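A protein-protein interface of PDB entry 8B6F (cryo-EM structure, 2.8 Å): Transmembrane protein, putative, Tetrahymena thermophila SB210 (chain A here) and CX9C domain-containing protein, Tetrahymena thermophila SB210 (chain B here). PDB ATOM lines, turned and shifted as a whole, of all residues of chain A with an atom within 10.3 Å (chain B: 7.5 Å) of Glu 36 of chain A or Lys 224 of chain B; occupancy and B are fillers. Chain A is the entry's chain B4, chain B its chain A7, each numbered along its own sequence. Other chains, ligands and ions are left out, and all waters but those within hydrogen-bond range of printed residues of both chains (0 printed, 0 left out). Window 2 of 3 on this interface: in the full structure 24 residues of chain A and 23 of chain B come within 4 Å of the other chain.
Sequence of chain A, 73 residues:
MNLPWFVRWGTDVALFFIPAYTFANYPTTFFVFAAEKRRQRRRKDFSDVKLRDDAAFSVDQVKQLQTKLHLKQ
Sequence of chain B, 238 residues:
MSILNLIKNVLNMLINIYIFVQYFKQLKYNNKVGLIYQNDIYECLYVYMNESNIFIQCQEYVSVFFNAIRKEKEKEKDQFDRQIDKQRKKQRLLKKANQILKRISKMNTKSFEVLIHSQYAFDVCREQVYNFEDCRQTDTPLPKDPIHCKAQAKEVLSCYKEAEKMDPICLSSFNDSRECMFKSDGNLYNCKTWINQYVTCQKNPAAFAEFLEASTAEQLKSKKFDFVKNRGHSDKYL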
ATOM      1  N   TYR A  26     -36.436 -11.485  11.486  1.00  0.00           N
ATOM      2  CA  TYR A  26     -35.626 -12.480  12.189  1.00  0.00           C
ATOM      3  C   TYR A  26     -36.529 -13.340  13.064  1.00  0.00           C
ATOM      4  O   TYR A  26     -36.520 -13.222  14.295  1.00  0.00           O
ATOM      5  CB  TYR A  26     -34.540 -11.797  13.021  1.00  0.00           C
ATOM      6  CG  TYR A  26     -33.530 -11.053  12.182  1.00  0.00           C
ATOM      7  CD1 TYR A  26     -32.400 -11.694  11.693  1.00  0.00           C
ATOM      8  CD2 TYR A  26     -33.710  -9.713  11.873  1.00  0.00           C
ATOM      9  CE1 TYR A  26     -31.475 -11.018  10.922  1.00  0.00           C
ATOM     10  CE2 TYR A  26     -32.791  -9.027  11.103  1.00  0.00           C
ATOM     11  CZ  TYR A  26     -31.675  -9.686  10.630  1.00  0.00           C
ATOM     12  OH  TYR A  26     -30.756  -9.011   9.863  1.00  0.00           O
ATOM     13  N   THR A  28     -36.210 -16.473  13.791  1.00  0.00           N
ATOM     14  CA  THR A  28     -35.355 -17.299  14.643  1.00  0.00           C
ATOM     15  C   THR A  28     -34.448 -16.369  15.445  1.00  0.00           C
ATOM     16  O   THR A  28     -33.272 -16.170  15.138  1.00  0.00           O
ATOM     17  CB  THR A  28     -34.553 -18.288  13.807  1.00  0.00           C
ATOM     18  OG1 THR A  28     -33.760 -17.578  12.847  1.00  0.00           O
ATOM     19  CG2 THR A  28     -35.480 -19.254  13.081  1.00  0.00           C
ATOM     20  N   PHE A  30     -32.002 -14.942  18.067  1.00  0.00           N
ATOM     21  CA  PHE A  30     -30.840 -15.376  18.834  1.00  0.00           C
ATOM     22  C   PHE A  30     -30.280 -16.710  18.358  1.00  0.00           C
ATOM     23  O   PHE A  30     -29.263 -17.160  18.898  1.00  0.00           O
ATOM     24  CB  PHE A  30     -31.146 -15.481  20.335  1.00  0.00           C
ATOM     25  CG  PHE A  30     -31.707 -14.219  20.926  1.00  0.00           C
ATOM     26  CD1 PHE A  30     -31.311 -12.977  20.450  1.00  0.00           C
ATOM     27  CD2 PHE A  30     -32.637 -14.274  21.951  1.00  0.00           C
ATOM     28  CE1 PHE A  30     -31.827 -11.815  20.989  1.00  0.00           C
ATOM     29  CE2 PHE A  30     -33.157 -13.115  22.495  1.00  0.00           C
ATOM     30  CZ  PHE A  30     -32.752 -11.883  22.014  1.00  0.00           C
ATOM     31  N   PHE A  31     -30.902 -17.356  17.374  1.00  0.00           N
ATOM     32  CA  PHE A  31     -30.376 -18.582  16.789  1.00  0.00           C
ATOM     33  C   PHE A  31     -29.866 -18.365  15.370  1.00  0.00           C
ATOM     34  O   PHE A  31     -29.555 -19.337  14.676  1.00  0.00           O
ATOM     35  CB  PHE A  31     -31.440 -19.680  16.806  1.00  0.00           C
ATOM     36  CG  PHE A  31     -31.782 -20.163  18.185  1.00  0.00           C
ATOM     37  CD1 PHE A  31     -31.017 -21.140  18.800  1.00  0.00           C
ATOM     38  CD2 PHE A  31     -32.868 -19.642  18.867  1.00  0.00           C
ATOM     39  CE1 PHE A  31     -31.329 -21.588  20.071  1.00  0.00           C
ATOM     40  CE2 PHE A  31     -33.185 -20.086  20.137  1.00  0.00           C
ATOM     41  CZ  PHE A  31     -32.415 -21.061  20.739  1.00  0.00           C
ATOM     42  N   VAL A  32     -29.775 -17.111  14.924  1.00  0.00           N
ATOM     43  CA  VAL A  32     -29.215 -16.829  13.606  1.00  0.00           C
ATOM     44  C   VAL A  32     -27.747 -17.226  13.565  1.00  0.00           C
ATOM     45  O   VAL A  32     -27.246 -17.718  12.548  1.00  0.00           O
ATOM     46  CB  VAL A  32     -29.409 -15.344  13.249  1.00  0.00           C
ATOM     47  CG1 VAL A  32     -28.912 -15.063  11.837  1.00  0.00           C
ATOM     48  CG2 VAL A  32     -30.870 -14.944  13.391  1.00  0.00           C
ATOM     49  N   PHE A  33     -27.034 -17.018  14.674  1.00  0.00           N
ATOM     50  CA  PHE A  33     -25.639 -17.436  14.745  1.00  0.00           C
ATOM     51  C   PHE A  33     -25.520 -18.950  14.656  1.00  0.00           C
ATOM     52  O   PHE A  33     -24.623 -19.473  13.984  1.00  0.00           O
ATOM     53  CB  PHE A  33     -25.004 -16.917  16.034  1.00  0.00           C
ATOM     54  CG  PHE A  33     -25.269 -15.462  16.292  1.00  0.00           C
ATOM     55  CD1 PHE A  33     -24.508 -14.487  15.672  1.00  0.00           C
ATOM     56  CD2 PHE A  33     -26.283 -15.070  17.151  1.00  0.00           C
ATOM     57  CE1 PHE A  33     -24.749 -13.147  15.905  1.00  0.00           C
ATOM     58  CE2 PHE A  33     -26.530 -13.733  17.388  1.00  0.00           C
ATOM     59  CZ  PHE A  33     -25.762 -12.769  16.765  1.00  0.00           C
ATOM     60  N   ALA A  34     -26.421 -19.672  15.323  1.00  0.00           N
ATOM     61  CA  ALA A  34     -26.431 -21.125  15.205  1.00  0.00           C
ATOM     62  C   ALA A  34     -26.720 -21.552  13.772  1.00  0.00           C
ATOM     63  O   ALA A  34     -26.138 -22.522  13.274  1.00  0.00           O
ATOM     64  CB  ALA A  34     -27.463 -21.722  16.161  1.00  0.00           C
ATOM     65  N   ALA A  35     -27.619 -20.838  13.092  1.00  0.00           N
ATOM     66  CA  ALA A  35     -27.898 -21.143  11.693  1.00  0.00           C
ATOM     67  C   ALA A  35     -26.663 -20.924  10.828  1.00  0.00           C
ATOM     68  O   ALA A  35     -26.374 -21.729   9.935  1.00  0.00           O
ATOM     69  CB  ALA A  35     -29.062 -20.288  11.192  1.00  0.00           C
ATOM     70  N   GLU A  36     -25.926 -19.839  11.074  1.00  0.00           N
ATOM     71  CA  GLU A  36     -24.694 -19.609  10.329  1.00  0.00           C
ATOM     72  C   GLU A  36     -23.692 -20.728  10.573  1.00  0.00           C
ATOM     73  O   GLU A  36     -23.049 -21.212   9.635  1.00  0.00           O
ATOM     74  CB  GLU A  36     -24.084 -18.262  10.719  1.00  0.00           C
ATOM     75  CG  GLU A  36     -24.885 -17.058  10.258  1.00  0.00           C
ATOM     76  CD  GLU A  36     -24.241 -15.746  10.666  1.00  0.00           C
ATOM     77  OE1 GLU A  36     -23.316 -15.772  11.504  1.00  0.00           O
ATOM     78  OE2 GLU A  36     -24.654 -14.689  10.143  1.00  0.00           O
ATOM     79  N   LYS A  37     -23.546 -21.153  11.829  1.00  0.00           N
ATOM     80  CA  LYS A  37     -22.624 -22.242  12.137  1.00  0.00           C
ATOM     81  C   LYS A  37     -23.055 -23.535  11.455  1.00  0.00           C
ATOM     82  O   LYS A  37     -22.216 -24.283  10.941  1.00  0.00           O
ATOM     83  CB  LYS A  37     -22.534 -22.436  13.650  1.00  0.00           C
ATOM     84  CG  LYS A  37     -21.900 -21.263  14.384  1.00  0.00           C
ATOM     85  CD  LYS A  37     -21.870 -21.505  15.885  1.00  0.00           C
ATOM     86  CE  LYS A  37     -21.218 -20.347  16.626  1.00  0.00           C
ATOM     87  NZ  LYS A  37     -21.975 -19.074  16.466  1.00  0.00           N
ATOM     88  N   ARG A  38     -24.359 -23.814  11.437  1.00  0.00           N
ATOM     89  CA  ARG A  38     -24.845 -25.016  10.768  1.00  0.00           C
ATOM     90  C   ARG A  38     -24.580 -24.955   9.270  1.00  0.00           C
ATOM     91  O   ARG A  38     -24.219 -25.964   8.654  1.00  0.00           O
ATOM     92  CB  ARG A  38     -26.335 -25.211  11.045  1.00  0.00           C
ATOM     93  CG  ARG A  38     -26.626 -25.713  12.451  1.00  0.00           C
ATOM     94  CD  ARG A  38     -28.072 -26.157  12.613  1.00  0.00           C
ATOM     95  NE  ARG A  38     -28.936 -25.082  13.090  1.00  0.00           N
ATOM     96  CZ  ARG A  38     -29.602 -24.244  12.308  1.00  0.00           C
ATOM     97  NH1 ARG A  38     -29.522 -24.313  10.990  1.00  0.00           N
ATOM     98  NH2 ARG A  38     -30.368 -23.309  12.864  1.00  0.00           N
ATOM     99  N   ARG A  39     -24.752 -23.780   8.664  1.00  0.00           N
ATOM    100  CA  ARG A  39     -24.430 -23.629   7.249  1.00  0.00           C
ATOM    101  C   ARG A  39     -22.948 -23.869   7.000  1.00  0.00           C
ATOM    102  O   ARG A  39     -22.573 -24.535   6.028  1.00  0.00           O
ATOM    103  CB  ARG A  39     -24.840 -22.239   6.764  1.00  0.00           C
ATOM    104  CG  ARG A  39     -24.686 -22.037   5.265  1.00  0.00           C
ATOM    105  CD  ARG A  39     -24.949 -20.595   4.874  1.00  0.00           C
ATOM    106  NE  ARG A  39     -23.955 -19.693   5.444  1.00  0.00           N
ATOM    107  CZ  ARG A  39     -22.793 -19.399   4.877  1.00  0.00           C
ATOM    108  NH1 ARG A  39     -22.439 -19.917   3.712  1.00  0.00           N
ATOM    109  NH2 ARG A  39     -21.961 -18.569   5.498  1.00  0.00           N
ATOM    110  N   GLN A  40     -22.086 -23.330   7.864  1.00  0.00           N
ATOM    111  CA  GLN A  40     -20.653 -23.563   7.723  1.00  0.00           C
ATOM    112  C   GLN A  40     -20.328 -25.047   7.825  1.00  0.00           C
ATOM    113  O   GLN A  40     -19.511 -25.567   7.055  1.00  0.00           O
ATOM    114  CB  GLN A  40     -19.889 -22.776   8.788  1.00  0.00           C
ATOM    115  CG  GLN A  40     -19.976 -21.266   8.631  1.00  0.00           C
ATOM    116  CD  GLN A  40     -19.184 -20.756   7.446  1.00  0.00           C
ATOM    117  OE1 GLN A  40     -18.669 -21.533   6.645  1.00  0.00           O
ATOM    118  NE2 GLN A  40     -19.079 -19.437   7.331  1.00  0.00           N
ATOM    119  N   ARG A  41     -20.955 -25.746   8.772  1.00  0.00           N
ATOM    120  CA  ARG A  41     -20.721 -27.180   8.915  1.00  0.00           C
ATOM    121  C   ARG A  41     -21.209 -27.944   7.691  1.00  0.00           C
ATOM    122  O   ARG A  41     -20.561 -28.899   7.250  1.00  0.00           O
ATOM    123  CB  ARG A  41     -21.397 -27.701  10.184  1.00  0.00           C
ATOM    124  CG  ARG A  41     -20.641 -27.365  11.464  1.00  0.00           C
ATOM    125  CD  ARG A  41     -21.278 -28.019  12.680  1.00  0.00           C
ATOM    126  NE  ARG A  41     -22.478 -27.317  13.121  1.00  0.00           N
ATOM    127  CZ  ARG A  41     -22.488 -26.320  13.995  1.00  0.00           C
ATOM    128  NH1 ARG A  41     -21.374 -25.868  14.545  1.00  0.00           N
ATOM    129  NH2 ARG A  41     -23.648 -25.759  14.325  1.00  0.00           N
ATOM    130  N   ARG A  42     -22.353 -27.544   7.129  1.00  0.00           N
ATOM    131  CA  ARG A  42     -22.847 -28.200   5.923  1.00  0.00           C
ATOM    132  C   ARG A  42     -21.882 -28.017   4.759  1.00  0.00           C
ATOM    133  O   ARG A  42     -21.712 -28.924   3.936  1.00  0.00           O
ATOM    134  CB  ARG A  42     -24.227 -27.662   5.550  1.00  0.00           C
ATOM    135  CG  ARG A  42     -25.351 -28.172   6.431  1.00  0.00           C
ATOM    136  CD  ARG A  42     -26.695 -27.995   5.746  1.00  0.00           C
ATOM    137  NE  ARG A  42     -26.891 -26.627   5.278  1.00  0.00           N
ATOM    138  CZ  ARG A  42     -27.386 -25.643   6.016  1.00  0.00           C
ATOM    139  NH1 ARG A  42     -27.748 -25.835   7.272  1.00  0.00           N
ATOM    140  NH2 ARG A  42     -27.525 -24.436   5.477  1.00  0.00           N
ATOM    141  N   ARG A  43     -21.256 -26.848   4.664  1.00  0.00           N
ATOM    142  CA  ARG A  43     -20.287 -26.600   3.605  1.00  0.00           C
ATOM    143  C   ARG A  43     -19.207 -27.673   3.620  1.00  0.00           C
ATOM    144  O   ARG A  43     -18.633 -27.981   4.667  1.00  0.00           O
ATOM    145  CB  ARG A  43     -19.669 -25.211   3.785  1.00  0.00           C
ATOM    146  CG  ARG A  43     -18.661 -24.837   2.714  1.00  0.00           C
ATOM    147  CD  ARG A  43     -18.311 -23.361   2.783  1.00  0.00           C
ATOM    148  NE  ARG A  43     -19.441 -22.520   2.408  1.00  0.00           N
ATOM    149  CZ  ARG A  43     -19.691 -22.092   1.177  1.00  0.00           C
ATOM    150  NH1 ARG A  43     -18.899 -22.397   0.163  1.00  0.00           N
ATOM    151  NH2 ARG A  43     -20.764 -21.337   0.959  1.00  0.00           N
ATOM    152  N   LYS A  72     -14.703 -15.213   1.250  1.00  0.00           N
ATOM    153  CA  LYS A  72     -15.779 -15.284   2.231  1.00  0.00           C
ATOM    154  C   LYS A  72     -15.527 -14.275   3.341  1.00  0.00           C
ATOM    155  O   LYS A  72     -14.456 -14.274   3.958  1.00  0.00           O
ATOM    156  CB  LYS A  72     -15.897 -16.693   2.813  1.00  0.00           C
ATOM    157  CG  LYS A  72     -16.522 -17.702   1.857  1.00  0.00           C
ATOM    158  CD  LYS A  72     -16.788 -19.038   2.541  1.00  0.00           C
ATOM    159  CE  LYS A  72     -15.501 -19.805   2.815  1.00  0.00           C
ATOM    160  NZ  LYS A  72     -14.807 -20.220   1.561  1.00  0.00           N
ATOM    161  N   GLN A  73     -16.515 -13.421   3.589  1.00  0.00           N
ATOM    162  CA  GLN A  73     -16.432 -12.428   4.651  1.00  0.00           C
ATOM    163  C   GLN A  73     -17.815 -12.150   5.229  1.00  0.00           C
ATOM    164  O   GLN A  73     -17.944 -11.576   6.310  1.00  0.00           O
ATOM    165  CB  GLN A  73     -15.809 -11.132   4.132  1.00  0.00           C
ATOM    166  CG  GLN A  73     -14.315 -11.227   3.871  1.00  0.00           C
ATOM    167  CD  GLN A  73     -13.702  -9.889   3.513  1.00  0.00           C
ATOM    168  OE1 GLN A  73     -14.324  -9.069   2.838  1.00  0.00           O
ATOM    169  NE2 GLN A  73     -12.478  -9.658   3.972  1.00  0.00           N
ATOM    170  OXT GLN A  73     -18.833 -12.491   4.628  1.00  0.00           O
ATOM    171  N   GLU B 179     -25.583 -25.344  -1.381  1.00  0.00           N
ATOM    172  CA  GLU B 179     -26.403 -24.547  -0.476  1.00  0.00           C
ATOM    173  C   GLU B 179     -27.670 -24.065  -1.169  1.00  0.00           C
ATOM    174  O   GLU B 179     -28.758 -24.098  -0.584  1.00  0.00           O
ATOM    175  CB  GLU B 179     -25.595 -23.362   0.051  1.00  0.00           C
ATOM    176  CG  GLU B 179     -26.377 -22.420   0.954  1.00  0.00           C
ATOM    177  CD  GLU B 179     -26.910 -23.105   2.194  1.00  0.00           C
ATOM    178  OE1 GLU B 179     -26.395 -24.186   2.548  1.00  0.00           O
ATOM    179  OE2 GLU B 179     -27.846 -22.562   2.815  1.00  0.00           O
ATOM    180  N   LYS B 183     -31.486 -25.035   0.069  1.00  0.00           N
ATOM    181  CA  LYS B 183     -32.507 -24.074   0.468  1.00  0.00           C
ATOM    182  C   LYS B 183     -33.724 -24.141  -0.447  1.00  0.00           C
ATOM    183  O   LYS B 183     -34.862 -24.016   0.020  1.00  0.00           O
ATOM    184  CB  LYS B 183     -31.909 -22.669   0.489  1.00  0.00           C
ATOM    185  CG  LYS B 183     -30.901 -22.458   1.615  1.00  0.00           C
ATOM    186  CD  LYS B 183     -31.556 -22.553   2.986  1.00  0.00           C
ATOM    187  CE  LYS B 183     -30.571 -22.217   4.091  1.00  0.00           C
ATOM    188  NZ  LYS B 183     -31.232 -22.177   5.423  1.00  0.00           N
ATOM    189  N   LYS B 221     -18.523 -12.264  -1.043  1.00  0.00           N
ATOM    190  CA  LYS B 221     -19.274 -12.246   0.203  1.00  0.00           C
ATOM    191  C   LYS B 221     -19.966 -13.585   0.391  1.00  0.00           C
ATOM    192  O   LYS B 221     -20.168 -14.344  -0.559  1.00  0.00           O
ATOM    193  CB  LYS B 221     -20.308 -11.112   0.230  1.00  0.00           C
ATOM    194  CG  LYS B 221     -19.711  -9.712   0.283  1.00  0.00           C
ATOM    195  CD  LYS B 221     -18.985  -9.462   1.600  1.00  0.00           C
ATOM    196  CE  LYS B 221     -18.427  -8.047   1.661  1.00  0.00           C
ATOM    197  NZ  LYS B 221     -17.718  -7.782   2.944  1.00  0.00           N
ATOM    198  N   SER B 222     -20.324 -13.866   1.641  1.00  0.00           N
ATOM    199  CA  SER B 222     -21.046 -15.090   1.954  1.00  0.00           C
ATOM    200  C   SER B 222     -22.397 -15.097   1.251  1.00  0.00           C
ATOM    201  O   SER B 222     -23.123 -14.100   1.260  1.00  0.00           O
ATOM    202  CB  SER B 222     -21.231 -15.208   3.465  1.00  0.00           C
ATOM    203  OG  SER B 222     -21.988 -16.356   3.799  1.00  0.00           O
ATOM    204  N   LYS B 223     -22.734 -16.233   0.644  1.00  0.00           N
ATOM    205  CA  LYS B 223     -23.963 -16.383  -0.128  1.00  0.00           C
ATOM    206  C   LYS B 223     -24.968 -17.177   0.698  1.00  0.00           C
ATOM    207  O   LYS B 223     -24.832 -18.395   0.851  1.00  0.00           O
ATOM    208  CB  LYS B 223     -23.678 -17.070  -1.462  1.00  0.00           C
ATOM    209  CG  LYS B 223     -22.722 -16.291  -2.355  1.00  0.00           C
ATOM    210  CD  LYS B 223     -22.266 -17.119  -3.544  1.00  0.00           C
ATOM    211  CE  LYS B 223     -21.280 -16.343  -4.405  1.00  0.00           C
ATOM    212  NZ  LYS B 223     -20.684 -17.192  -5.478  1.00  0.00           N
ATOM    213  N   LYS B 224     -25.975 -16.487   1.224  1.00  0.00           N
ATOM    214  CA  LYS B 224     -27.032 -17.098   2.015  1.00  0.00           C
ATOM    215  C   LYS B 224     -28.332 -17.048   1.226  1.00  0.00           C
ATOM    216  O   LYS B 224     -28.708 -15.989   0.711  1.00  0.00           O
ATOM    217  CB  LYS B 224     -27.197 -16.379   3.355  1.00  0.00           C
ATOM    218  CG  LYS B 224     -25.927 -16.335   4.187  1.00  0.00           C
ATOM    219  CD  LYS B 224     -26.140 -15.551   5.472  1.00  0.00           C
ATOM    220  CE  LYS B 224     -24.874 -15.501   6.308  1.00  0.00           C
ATOM    221  NZ  LYS B 224     -24.409 -16.860   6.701  1.00  0.00           N
ATOM    222  N   PHE B 225     -29.015 -18.184   1.138  1.00  0.00           N
ATOM    223  CA  PHE B 225     -30.240 -18.310   0.359  1.00  0.00           C
ATOM    224  C   PHE B 225     -31.423 -18.502   1.296  1.00  0.00           C
ATOM    225  O   PHE B 225     -31.383 -19.354   2.189  1.00  0.00           O
ATOM    226  CB  PHE B 225     -30.148 -19.480  -0.623  1.00  0.00           C
ATOM    227  CG  PHE B 225     -28.990 -19.385  -1.571  1.00  0.00           C
ATOM    228  CD1 PHE B 225     -27.735 -19.835  -1.199  1.00  0.00           C
ATOM    229  CD2 PHE B 225     -29.157 -18.854  -2.838  1.00  0.00           C
ATOM    230  CE1 PHE B 225     -26.667 -19.752  -2.070  1.00  0.00           C
ATOM    231  CE2 PHE B 225     -28.096 -18.768  -3.713  1.00  0.00           C
ATOM    232  CZ  PHE B 225     -26.848 -19.218  -3.330  1.00  0.00           C
ATOM    233  N   ASP B 226     -32.468 -17.701   1.094  1.00  0.00           N
ATOM    234  CA  ASP B 226     -33.716 -17.815   1.848  1.00  0.00           C
ATOM    235  C   ASP B 226     -34.852 -17.500   0.881  1.00  0.00           C
ATOM    236  O   ASP B 226     -35.182 -16.331   0.665  1.00  0.00           O
ATOM    237  CB  ASP B 226     -33.730 -16.876   3.047  1.00  0.00           C
ATOM    238  CG  ASP B 226     -35.023 -16.953   3.834  1.00  0.00           C
ATOM    239  OD1 ASP B 226     -35.829 -17.870   3.571  1.00  0.00           O
ATOM    240  OD2 ASP B 226     -35.236 -16.094   4.713  1.00  0.00           O
ATOM    241  N   PHE B 227     -35.448 -18.544   0.304  1.00  0.00           N
ATOM    242  CA  PHE B 227     -36.440 -18.336  -0.746  1.00  0.00           C
ATOM    243  C   PHE B 227     -37.769 -17.846  -0.186  1.00  0.00           C
ATOM    244  O   PHE B 227     -38.522 -17.170  -0.894  1.00  0.00           O
ATOM    245  CB  PHE B 227     -36.621 -19.625  -1.548  1.00  0.00           C
ATOM    246  CG  PHE B 227     -35.437 -19.960  -2.412  1.00  0.00           C
ATOM    247  CD1 PHE B 227     -34.290 -20.504  -1.858  1.00  0.00           C
ATOM    248  CD2 PHE B 227     -35.464 -19.713  -3.775  1.00  0.00           C
ATOM    249  CE1 PHE B 227     -33.196 -20.805  -2.648  1.00  0.00           C
ATOM    250  CE2 PHE B 227     -34.372 -20.010  -4.570  1.00  0.00           C
ATOM    251  CZ  PHE B 227     -33.238 -20.557  -4.006  1.00  0.00           C
ATOM    252  N   ASN B 230     -37.086 -14.270  -0.071  1.00  0.00           N
ATOM    253  CA  ASN B 230     -36.886 -13.817  -1.447  1.00  0.00           C
ATOM    254  C   ASN B 230     -37.444 -14.882  -2.386  1.00  0.00           C
ATOM    255  O   ASN B 230     -36.713 -15.745  -2.874  1.00  0.00           O
ATOM    256  CB  ASN B 230     -35.409 -13.555  -1.711  1.00  0.00           C
ATOM    257  CG  ASN B 230     -34.754 -12.754  -0.606  1.00  0.00           C
ATOM    258  OD1 ASN B 230     -35.369 -11.867  -0.020  1.00  0.00           O
ATOM    259  ND2 ASN B 230     -33.497 -13.066  -0.315  1.00  0.00           N
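Along chain B the printed residues that touch a printed residue of chain A span positions 179 to 224.
Among the printed residues, 7 pairs touch across the chains.
Among the printed residues, Asp or Glu carboxylates within 4 Å of a Lys or Arg side-chain nitrogen of the other chain: Arg 42 of chain A with Glu 179 of chain B (3.1 Å).
The side-chain hydroxyl (OG) of Ser 222 of chain B sits at hydrogen-bond distance from the guanidinium group (NH2) of Arg 39 of chain A (2.8 Å).
The guanidinium group (NH2) of Arg 42 of chain A is in salt-bridge range of the side-chain carboxylate (OE1) of Glu 179 of chain B.
The guanidinium group (NE) of Arg 39 of chain A sits close to the side-chain amino group (NZ) of Lys 224 of chain B (3.1 Å).
Glu 36 of chain A touches Lys 224 of chain B.
Glu 179 of chain B touches Arg 39 of chain A.
Lys 221 of chain B touches Gln 73 of chain A (NZ to OE1, 3.6 Å).
OXT of Gln 73 of chain A touches N of Ser 222 of chain B (3.6 Å).
Of chain A, only Glu 36 and Arg 39 come within 4 Å of Lys 224 of chain B.
No residue of chain B comes within 4 Å of Ala 35 of chain A.
Of the printed residues of chain A, Ser 222 of chain B touches Arg 39 and Gln 73.
Of the printed residues of chain A, Glu 179 of chain B touches Arg 39 and Arg 42.
Of the printed residues of chain B, Arg 42 of chain A touches Glu 179 (3.1 Å).
Of the printed residues of chain B, Arg 39 of chain A touches Glu 179, Ser 222 and Lys 224.
Lys 183 of chain B touches none of the printed residues of chain A.
Phe 227 of chain B touches none of the printed residues of chain A.
The nearest residue of chain B that does not touch Glu 36 of chain A is Ser 222 of chain B (7.1 Å).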
